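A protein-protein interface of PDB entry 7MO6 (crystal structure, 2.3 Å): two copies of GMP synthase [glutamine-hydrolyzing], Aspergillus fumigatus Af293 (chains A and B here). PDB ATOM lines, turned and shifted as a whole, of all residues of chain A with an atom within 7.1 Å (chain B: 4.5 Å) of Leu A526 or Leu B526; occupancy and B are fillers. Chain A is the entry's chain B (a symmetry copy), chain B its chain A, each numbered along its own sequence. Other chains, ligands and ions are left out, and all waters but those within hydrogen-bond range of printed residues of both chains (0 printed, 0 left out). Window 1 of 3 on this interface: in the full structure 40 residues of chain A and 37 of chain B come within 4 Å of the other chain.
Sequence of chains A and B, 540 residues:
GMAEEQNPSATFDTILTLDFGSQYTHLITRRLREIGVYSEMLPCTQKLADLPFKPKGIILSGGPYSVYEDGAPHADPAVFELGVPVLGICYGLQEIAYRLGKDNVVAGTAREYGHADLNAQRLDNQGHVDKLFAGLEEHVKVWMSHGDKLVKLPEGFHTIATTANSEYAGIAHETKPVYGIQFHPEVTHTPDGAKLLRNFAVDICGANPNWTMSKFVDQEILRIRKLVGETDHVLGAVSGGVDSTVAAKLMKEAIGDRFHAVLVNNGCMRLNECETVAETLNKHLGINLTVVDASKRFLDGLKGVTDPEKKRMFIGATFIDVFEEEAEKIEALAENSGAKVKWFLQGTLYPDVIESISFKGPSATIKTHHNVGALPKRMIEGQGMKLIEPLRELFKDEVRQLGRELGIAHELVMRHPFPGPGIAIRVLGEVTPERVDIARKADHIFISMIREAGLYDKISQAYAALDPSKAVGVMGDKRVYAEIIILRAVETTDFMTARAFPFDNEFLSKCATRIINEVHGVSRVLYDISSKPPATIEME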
ATOM      1  N   LEU A 428      15.213  34.767   5.609  1.00  0.00           N
ATOM      2  CA  LEU A 428      15.677  35.370   6.850  1.00  0.00           C
ATOM      3  C   LEU A 428      17.165  35.687   6.753  1.00  0.00           C
ATOM      4  O   LEU A 428      17.973  34.824   6.401  1.00  0.00           O
ATOM      5  CB  LEU A 428      15.398  34.437   8.031  1.00  0.00           C
ATOM      6  CG  LEU A 428      13.943  34.284   8.499  1.00  0.00           C
ATOM      7  CD1 LEU A 428      13.096  33.471   7.528  1.00  0.00           C
ATOM      8  CD2 LEU A 428      13.885  33.664   9.883  1.00  0.00           C
ATOM      9  N   ALA A 465       9.511  29.937   3.646  1.00  0.00           N
ATOM     10  CA  ALA A 465      10.642  30.826   3.853  1.00  0.00           C
ATOM     11  C   ALA A 465      11.885  30.014   4.188  1.00  0.00           C
ATOM     12  O   ALA A 465      11.805  28.958   4.822  1.00  0.00           O
ATOM     13  CB  ALA A 465      10.360  31.835   4.975  1.00  0.00           C
ATOM     14  N   ASP A 467      15.406  29.501   6.154  1.00  0.00           N
ATOM     15  CA  ASP A 467      16.071  29.865   7.393  1.00  0.00           C
ATOM     16  C   ASP A 467      17.544  29.502   7.281  1.00  0.00           C
ATOM     17  O   ASP A 467      17.871  28.314   7.150  1.00  0.00           O
ATOM     18  CB  ASP A 467      15.429  29.146   8.579  1.00  0.00           C
ATOM     19  CG  ASP A 467      15.722  29.822   9.903  1.00  0.00           C
ATOM     20  OD1 ASP A 467      16.860  30.294  10.105  1.00  0.00           O
ATOM     21  OD2 ASP A 467      14.804  29.882  10.747  1.00  0.00           O
ATOM     22  N   ILE A 484      17.119  25.542   6.581  1.00  0.00           N
ATOM     23  CA  ILE A 484      15.814  25.144   7.093  1.00  0.00           C
ATOM     24  C   ILE A 484      14.726  25.856   6.303  1.00  0.00           C
ATOM     25  O   ILE A 484      14.855  27.042   5.979  1.00  0.00           O
ATOM     26  CB  ILE A 484      15.689  25.456   8.600  1.00  0.00           C
ATOM     27  CG1 ILE A 484      16.748  24.688   9.391  1.00  0.00           C
ATOM     28  CG2 ILE A 484      14.296  25.128   9.110  1.00  0.00           C
ATOM     29  CD1 ILE A 484      16.734  24.981  10.876  1.00  0.00           C
ATOM     30  N   ILE A 485      13.657  25.128   5.989  1.00  0.00           N
ATOM     31  CA  ILE A 485      12.476  25.684   5.341  1.00  0.00           C
ATOM     32  C   ILE A 485      11.391  25.871   6.393  1.00  0.00           C
ATOM     33  O   ILE A 485      11.101  24.951   7.167  1.00  0.00           O
ATOM     34  CB  ILE A 485      11.987  24.777   4.198  1.00  0.00           C
ATOM     35  CG1 ILE A 485      12.917  24.895   2.991  1.00  0.00           C
ATOM     36  CG2 ILE A 485      10.555  25.120   3.812  1.00  0.00           C
ATOM     37  CD1 ILE A 485      13.076  26.309   2.477  1.00  0.00           C
ATOM     38  N   ILE A 486      10.799  27.062   6.427  1.00  0.00           N
ATOM     39  CA  ILE A 486       9.709  27.385   7.340  1.00  0.00           C
ATOM     40  C   ILE A 486       8.433  27.530   6.526  1.00  0.00           C
ATOM     41  O   ILE A 486       8.388  28.310   5.568  1.00  0.00           O
ATOM     42  CB  ILE A 486       9.997  28.670   8.136  1.00  0.00           C
ATOM     43  CG1 ILE A 486      11.363  28.586   8.817  1.00  0.00           C
ATOM     44  CG2 ILE A 486       8.900  28.915   9.160  1.00  0.00           C
ATOM     45  CD1 ILE A 486      11.785  29.875   9.490  1.00  0.00           C
ATOM     46  N   LEU A 487       7.402  26.780   6.901  1.00  0.00           N
ATOM     47  CA  LEU A 487       6.100  26.855   6.254  1.00  0.00           C
ATOM     48  C   LEU A 487       5.179  27.775   7.047  1.00  0.00           C
ATOM     49  O   LEU A 487       5.149  27.731   8.280  1.00  0.00           O
ATOM     50  CB  LEU A 487       5.468  25.468   6.122  1.00  0.00           C
ATOM     51  CG  LEU A 487       6.216  24.444   5.263  1.00  0.00           C
ATOM     52  CD1 LEU A 487       5.424  23.148   5.164  1.00  0.00           C
ATOM     53  CD2 LEU A 487       6.513  25.001   3.878  1.00  0.00           C
ATOM     54  N   ARG A 488       4.425  28.605   6.330  1.00  0.00           N
ATOM     55  CA  ARG A 488       3.543  29.584   6.951  1.00  0.00           C
ATOM     56  C   ARG A 488       2.200  29.569   6.242  1.00  0.00           C
ATOM     57  O   ARG A 488       2.149  29.620   5.009  1.00  0.00           O
ATOM     58  CB  ARG A 488       4.162  30.986   6.901  1.00  0.00           C
ATOM     59  CG  ARG A 488       3.299  32.085   7.502  1.00  0.00           C
ATOM     60  CD  ARG A 488       2.881  31.756   8.922  1.00  0.00           C
ATOM     61  NE  ARG A 488       2.892  32.935   9.782  1.00  0.00           N
ATOM     62  CZ  ARG A 488       2.355  32.977  10.997  1.00  0.00           C
ATOM     63  NH1 ARG A 488       1.748  31.908  11.493  1.00  0.00           N
ATOM     64  NH2 ARG A 488       2.418  34.090  11.713  1.00  0.00           N
ATOM     65  N   ALA A 512       6.409  18.026   4.350  1.00  0.00           N
ATOM     66  CA  ALA A 512       7.766  18.166   4.869  1.00  0.00           C
ATOM     67  C   ALA A 512       8.695  17.122   4.265  1.00  0.00           C
ATOM     68  O   ALA A 512       9.871  17.405   4.005  1.00  0.00           O
ATOM     69  CB  ALA A 512       7.760  18.062   6.393  1.00  0.00           C
ATOM     70  N   ARG A 524      15.565  20.424   7.388  1.00  0.00           N
ATOM     71  CA  ARG A 524      14.384  20.385   8.238  1.00  0.00           C
ATOM     72  C   ARG A 524      13.300  21.276   7.650  1.00  0.00           C
ATOM     73  O   ARG A 524      13.586  22.258   6.961  1.00  0.00           O
ATOM     74  CB  ARG A 524      14.690  20.840   9.671  1.00  0.00           C
ATOM     75  CG  ARG A 524      15.632  19.931  10.438  1.00  0.00           C
ATOM     76  CD  ARG A 524      14.964  18.635  10.849  1.00  0.00           C
ATOM     77  NE  ARG A 524      15.034  18.438  12.294  1.00  0.00           N
ATOM     78  CZ  ARG A 524      16.100  17.964  12.931  1.00  0.00           C
ATOM     79  NH1 ARG A 524      16.076  17.822  14.247  1.00  0.00           N
ATOM     80  NH2 ARG A 524      17.190  17.633  12.252  1.00  0.00           N
ATOM     81  N   VAL A 525      12.050  20.923   7.939  1.00  0.00           N
ATOM     82  CA  VAL A 525      10.889  21.720   7.562  1.00  0.00           C
ATOM     83  C   VAL A 525      10.105  22.032   8.828  1.00  0.00           C
ATOM     84  O   VAL A 525       9.766  21.123   9.595  1.00  0.00           O
ATOM     85  CB  VAL A 525      10.003  20.993   6.535  1.00  0.00           C
ATOM     86  CG1 VAL A 525       8.813  21.858   6.157  1.00  0.00           C
ATOM     87  CG2 VAL A 525      10.811  20.626   5.301  1.00  0.00           C
ATOM     88  N   LEU A 526       9.826  23.314   9.047  1.00  0.00           N
ATOM     89  CA  LEU A 526       9.118  23.777  10.229  1.00  0.00           C
ATOM     90  C   LEU A 526       7.825  24.463   9.817  1.00  0.00           C
ATOM     91  O   LEU A 526       7.784  25.174   8.808  1.00  0.00           O
ATOM     92  CB  LEU A 526       9.980  24.745  11.048  1.00  0.00           C
ATOM     93  CG  LEU A 526      11.443  24.365  11.282  1.00  0.00           C
ATOM     94  CD1 LEU A 526      12.147  25.439  12.099  1.00  0.00           C
ATOM     95  CD2 LEU A 526      11.564  23.010  11.959  1.00  0.00           C
ATOM     96  N   TYR A 527       6.770  24.249  10.598  1.00  0.00           N
ATOM     97  CA  TYR A 527       5.483  24.894  10.374  1.00  0.00           C
ATOM     98  C   TYR A 527       5.279  25.962  11.437  1.00  0.00           C
ATOM     99  O   TYR A 527       5.336  25.670  12.636  1.00  0.00           O
ATOM    100  CB  TYR A 527       4.338  23.881  10.402  1.00  0.00           C
ATOM    101  CG  TYR A 527       2.977  24.504  10.178  1.00  0.00           C
ATOM    102  CD1 TYR A 527       2.738  25.315   9.075  1.00  0.00           C
ATOM    103  CD2 TYR A 527       1.932  24.275  11.062  1.00  0.00           C
ATOM    104  CE1 TYR A 527       1.497  25.885   8.860  1.00  0.00           C
ATOM    105  CE2 TYR A 527       0.685  24.842  10.856  1.00  0.00           C
ATOM    106  CZ  TYR A 527       0.474  25.646   9.754  1.00  0.00           C
ATOM    107  OH  TYR A 527      -0.763  26.212   9.543  1.00  0.00           O
ATOM    108  N   ASP A 528       5.046  27.196  10.996  1.00  0.00           N
ATOM    109  CA  ASP A 528       4.808  28.301  11.913  1.00  0.00           C
ATOM    110  C   ASP A 528       3.441  28.136  12.566  1.00  0.00           C
ATOM    111  O   ASP A 528       2.422  28.040  11.873  1.00  0.00           O
ATOM    112  CB  ASP A 528       4.898  29.630  11.166  1.00  0.00           C
ATOM    113  CG  ASP A 528       5.022  30.827  12.098  1.00  0.00           C
ATOM    114  OD1 ASP A 528       4.481  30.779  13.223  1.00  0.00           O
ATOM    115  OD2 ASP A 528       5.664  31.823  11.703  1.00  0.00           O
ATOM    116  N   ILE A 529       3.416  28.098  13.897  1.00  0.00           N
ATOM    117  CA  ILE A 529       2.180  27.966  14.656  1.00  0.00           C
ATOM    118  C   ILE A 529       1.819  29.256  15.382  1.00  0.00           C
ATOM    119  O   ILE A 529       0.890  29.265  16.196  1.00  0.00           O
ATOM    120  CB  ILE A 529       2.251  26.786  15.640  1.00  0.00           C
ATOM    121  CG1 ILE A 529       3.451  26.938  16.577  1.00  0.00           C
ATOM    122  CG2 ILE A 529       2.324  25.468  14.887  1.00  0.00           C
ATOM    123  CD1 ILE A 529       3.605  25.802  17.566  1.00  0.00           C
ATOM    124  N   SER A 530       2.528  30.348  15.107  1.00  0.00           N
ATOM    125  CA  SER A 530       2.230  31.619  15.753  1.00  0.00           C
ATOM    126  C   SER A 530       0.979  32.243  15.144  1.00  0.00           C
ATOM    127  O   SER A 530       0.851  32.337  13.919  1.00  0.00           O
ATOM    128  CB  SER A 530       3.412  32.576  15.620  1.00  0.00           C
ATOM    129  OG  SER A 530       4.588  32.018  16.181  1.00  0.00           O
ATOM    130  N   MET A 539       7.538  37.106   7.689  1.00  0.00           N
ATOM    131  CA  MET A 539       8.703  36.855   8.529  1.00  0.00           C
ATOM    132  C   MET A 539       9.528  38.107   8.791  1.00  0.00           C
ATOM    133  O   MET A 539      10.147  38.216   9.856  1.00  0.00           O
ATOM    134  CB  MET A 539       9.592  35.781   7.893  1.00  0.00           C
ATOM    135  CG  MET A 539       8.934  34.415   7.808  1.00  0.00           C
ATOM    136  SD  MET A 539       8.515  33.751   9.431  1.00  0.00           S
ATOM    137  CE  MET A 539       7.503  32.349   8.967  1.00  0.00           C
ATOM    138  N   ILE B 484      13.790  33.155  17.483  1.00  0.00           N
ATOM    139  CA  ILE B 484      12.772  32.165  17.161  1.00  0.00           C
ATOM    140  C   ILE B 484      12.945  30.956  18.069  1.00  0.00           C
ATOM    141  O   ILE B 484      14.073  30.536  18.350  1.00  0.00           O
ATOM    142  CB  ILE B 484      12.851  31.753  15.675  1.00  0.00           C
ATOM    143  CG1 ILE B 484      12.636  32.970  14.773  1.00  0.00           C
ATOM    144  CG2 ILE B 484      11.843  30.659  15.356  1.00  0.00           C
ATOM    145  CD1 ILE B 484      12.876  32.694  13.308  1.00  0.00           C
ATOM    146  N   ILE B 485      11.825  30.402  18.528  1.00  0.00           N
ATOM    147  CA  ILE B 485      11.800  29.170  19.308  1.00  0.00           C
ATOM    148  C   ILE B 485      11.273  28.054  18.417  1.00  0.00           C
ATOM    149  O   ILE B 485      10.266  28.230  17.720  1.00  0.00           O
ATOM    150  CB  ILE B 485      10.942  29.320  20.577  1.00  0.00           C
ATOM    151  CG1 ILE B 485      11.653  30.210  21.599  1.00  0.00           C
ATOM    152  CG2 ILE B 485      10.626  27.960  21.182  1.00  0.00           C
ATOM    153  CD1 ILE B 485      12.988  29.669  22.060  1.00  0.00           C
ATOM    154  N   ILE B 486      11.956  26.913  18.435  1.00  0.00           N
ATOM    155  CA  ILE B 486      11.591  25.754  17.629  1.00  0.00           C
ATOM    156  C   ILE B 486      11.156  24.640  18.570  1.00  0.00           C
ATOM    157  O   ILE B 486      11.930  24.207  19.433  1.00  0.00           O
ATOM    158  CB  ILE B 486      12.752  25.295  16.736  1.00  0.00           C
ATOM    159  CG1 ILE B 486      13.174  26.418  15.785  1.00  0.00           C
ATOM    160  CG2 ILE B 486      12.364  24.047  15.956  1.00  0.00           C
ATOM    161  CD1 ILE B 486      14.368  26.070  14.922  1.00  0.00           C
ATOM    162  N   LEU B 487       9.919  24.177  18.407  1.00  0.00           N
ATOM    163  CA  LEU B 487       9.401  23.065  19.189  1.00  0.00           C
ATOM    164  C   LEU B 487       9.627  21.755  18.447  1.00  0.00           C
ATOM    165  O   LEU B 487       9.496  21.688  17.221  1.00  0.00           O
ATOM    166  CB  LEU B 487       7.912  23.252  19.484  1.00  0.00           C
ATOM    167  CG  LEU B 487       7.537  24.473  20.329  1.00  0.00           C
ATOM    168  CD1 LEU B 487       6.048  24.472  20.633  1.00  0.00           C
ATOM    169  CD2 LEU B 487       8.352  24.517  21.614  1.00  0.00           C
ATOM    170  N   ARG B 524       8.632  34.460  17.332  1.00  0.00           N
ATOM    171  CA  ARG B 524       8.001  33.395  16.566  1.00  0.00           C
ATOM    172  C   ARG B 524       8.202  32.059  17.266  1.00  0.00           C
ATOM    173  O   ARG B 524       9.212  31.834  17.937  1.00  0.00           O
ATOM    174  CB  ARG B 524       8.559  33.312  15.138  1.00  0.00           C
ATOM    175  CG  ARG B 524       8.016  34.366  14.192  1.00  0.00           C
ATOM    176  CD  ARG B 524       6.510  34.245  14.032  1.00  0.00           C
ATOM    177  NE  ARG B 524       6.120  34.131  12.631  1.00  0.00           N
ATOM    178  CZ  ARG B 524       5.951  35.166  11.814  1.00  0.00           C
ATOM    179  NH1 ARG B 524       6.141  36.401  12.256  1.00  0.00           N
ATOM    180  NH2 ARG B 524       5.596  34.965  10.552  1.00  0.00           N
ATOM    181  N   VAL B 525       7.223  31.172  17.094  1.00  0.00           N
ATOM    182  CA  VAL B 525       7.280  29.807  17.606  1.00  0.00           C
ATOM    183  C   VAL B 525       6.960  28.867  16.452  1.00  0.00           C
ATOM    184  O   VAL B 525       5.875  28.948  15.864  1.00  0.00           O
ATOM    185  CB  VAL B 525       6.304  29.581  18.773  1.00  0.00           C
ATOM    186  CG1 VAL B 525       6.228  28.101  19.121  1.00  0.00           C
ATOM    187  CG2 VAL B 525       6.731  30.394  19.985  1.00  0.00           C
ATOM    188  N   LEU B 526       7.899  27.983  16.127  1.00  0.00           N
ATOM    189  CA  LEU B 526       7.742  27.031  15.038  1.00  0.00           C
ATOM    190  C   LEU B 526       7.754  25.613  15.589  1.00  0.00           C
ATOM    191  O   LEU B 526       8.365  25.339  16.627  1.00  0.00           O
ATOM    192  CB  LEU B 526       8.854  27.191  13.994  1.00  0.00           C
ATOM    193  CG  LEU B 526       9.261  28.620  13.626  1.00  0.00           C
ATOM    194  CD1 LEU B 526      10.392  28.602  12.615  1.00  0.00           C
ATOM    195  CD2 LEU B 526       8.079  29.415  13.095  1.00  0.00           C
ATOM    196  N   TYR B 527       7.074  24.710  14.886  1.00  0.00           N
ATOM    197  CA  TYR B 527       7.001  23.307  15.269  1.00  0.00           C
ATOM    198  C   TYR B 527       7.635  22.453  14.182  1.00  0.00           C
ATOM    199  O   TYR B 527       7.258  22.551  13.010  1.00  0.00           O
ATOM    200  CB  TYR B 527       5.554  22.870  15.514  1.00  0.00           C
ATOM    201  CG  TYR B 527       5.417  21.418  15.911  1.00  0.00           C
ATOM    202  CD1 TYR B 527       6.229  20.867  16.894  1.00  0.00           C
ATOM    203  CD2 TYR B 527       4.468  20.601  15.314  1.00  0.00           C
ATOM    204  CE1 TYR B 527       6.107  19.542  17.264  1.00  0.00           C
ATOM    205  CE2 TYR B 527       4.336  19.274  15.677  1.00  0.00           C
ATOM    206  CZ  TYR B 527       5.158  18.751  16.652  1.00  0.00           C
ATOM    207  OH  TYR B 527       5.030  17.430  17.017  1.00  0.00           O
ATOM    208  N   ASP B 528       8.597  21.621  14.574  1.00  0.00           N
ATOM    209  CA  ASP B 528       9.283  20.755  13.625  1.00  0.00           C
ATOM    210  C   ASP B 528       8.352  19.630  13.185  1.00  0.00           C
ATOM    211  O   ASP B 528       7.815  18.895  14.022  1.00  0.00           O
ATOM    212  CB  ASP B 528      10.557  20.193  14.252  1.00  0.00           C
ATOM    213  CG  ASP B 528      11.466  19.521  13.238  1.00  0.00           C
ATOM    214  OD1 ASP B 528      11.078  19.417  12.056  1.00  0.00           O
ATOM    215  OD2 ASP B 528      12.577  19.100  13.624  1.00  0.00           O
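Among the printed residues, pairs that only touch across the chains: Asp A528 with Val B525 (3.5 Å), Asp A528 with Leu B526 (3.5 Å), Leu A526 with Tyr B527 (3.6 Å), Leu A526 with Asp B528 (3.6 Å), Ser A530 with Arg B524 (3.6 Å), Leu A526 with Ile B486 (3.6 Å), Ile A486 with Leu B526 (3.7 Å), Leu A526 with Leu B526 (3.7 Å), Tyr A527 with Leu B526 (3.7 Å) and Leu A428 with Ile B484 (3.7 Å).
NH1 of Arg A488 is in hydrogen-bond range of O of Ser A530 (2.6 Å).
NH1 of Arg A488 is in salt-bridge range of OD1 of Asp A528 (3.4 Å).
The backbone carbonyl oxygen of Leu A487 lies within hydrogen-bond range of the backbone NH of Asp A528 (2.8 Å).
The backbone NH (N) of Leu B487 lies within hydrogen-bond range of the backbone carbonyl oxygen (O) of Leu B526, at 2.6 Å.
The backbone NH of Ile B485 lies within hydrogen-bond range of the backbone carbonyl oxygen of Arg B524 (3.0 Å).
The backbone carbonyl oxygen (O) of Ile B485 is in hydrogen-bond range of the backbone NH (N) of Leu B526 (2.9 Å).
Hydrophobic or aromatic side chains of chain B that line the printed part of chain A: Ile B484, Ile B486, Val B525 and Leu B526.
Hydrophobic or aromatic side chains of chain A that line the printed part of chain B: Leu A428, Ile A486, Leu A526, Ile A529 and Met A539.
Along chain A the printed residues that touch a printed residue of chain B span positions 428 to 539.
Among the printed residues, 18 pairs touch across the chains.
Among the printed residues, Asp or Glu carboxylates within 4 Å of a Lys or Arg side-chain nitrogen of the other chain: Arg A524 with Asp B528 and Asp A528 with Arg B524.
Arg A524 touches Asp B528, and with the chains exchanged Asp A528 touches Arg B524.
Leu B526 touches its own counterpart, Leu A526.
Leu A526 touches Tyr B527, and with the chains exchanged Tyr A527 touches Leu B526.
Tyr B527 touches its own counterpart, Tyr A527.
Of the 18 pairs that touch across the chains among the printed residues, 12 have their exchanged pair printed and touching as well.
The backbone carbonyl oxygen of Val B525 lies close to the backbone NH of Ile A529.
The side-chain carboxylate (OD2) of Asp A528 lies within salt-bridge range of the guanidinium group (NE) of Arg B524, 2.5 Å away.
The backbone NH (N) of Val B525 sits at hydrogen-bond distance from the side-chain hydroxyl (OG) of Ser A530, 2.9 Å away.
NE of Arg A524 is in salt-bridge range of OD2 of Asp B528 (2.9 Å).
The side-chain carboxylate (OD1) of Asp B528 sits close to the backbone carbonyl oxygen (O) of Val A525, at 3.3 Å.
The side-chain sulfur of Met A539 is in hydrogen-bond range of the guanidinium group of Arg B524 (3.4 Å).
The guanidinium group of Arg A488 sits close to the guanidinium group of Arg B524 (3.5 Å).
O of Tyr B527 sits at hydrogen-bond distance from N of Tyr A527 (3.0 Å).
Of the printed residues of chain B, Arg A488 touches Arg B524.
Ala A512 touches none of the printed residues of chain B.
Printed residues of chain B within 4 Å of Val A525: Asp B528 (3.3 Å).
Leu A526 touches four residues of chain B.
Printed residues of chain B within 4 Å of Asp A528: Arg B524 (2.5 Å), Val B525 (3.5 Å) and Leu B526 (3.5 Å).
Leu B487 touches none of the printed residues of chain A.
Of the printed residues of chain A, Arg B524 touches Arg A488 (3.5 Å), Asp A528 (2.5 Å), Ser A530 (3.6 Å) and Met A539 (3.4 Å).
Of the printed residues of chain A, Leu B526 touches Ile A486, Leu A526, Tyr A527 and Asp A528.
Of the printed residues of chain A, Asp B528 touches Arg A524, Val A525 and Leu A526.
The nearest printed residue of chain B that does not touch Leu A526 is Leu B487 (5.8 Å).
The nearest printed residue of chain A that does not touch Ile B484 is Asp A467 (4.3 Å).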
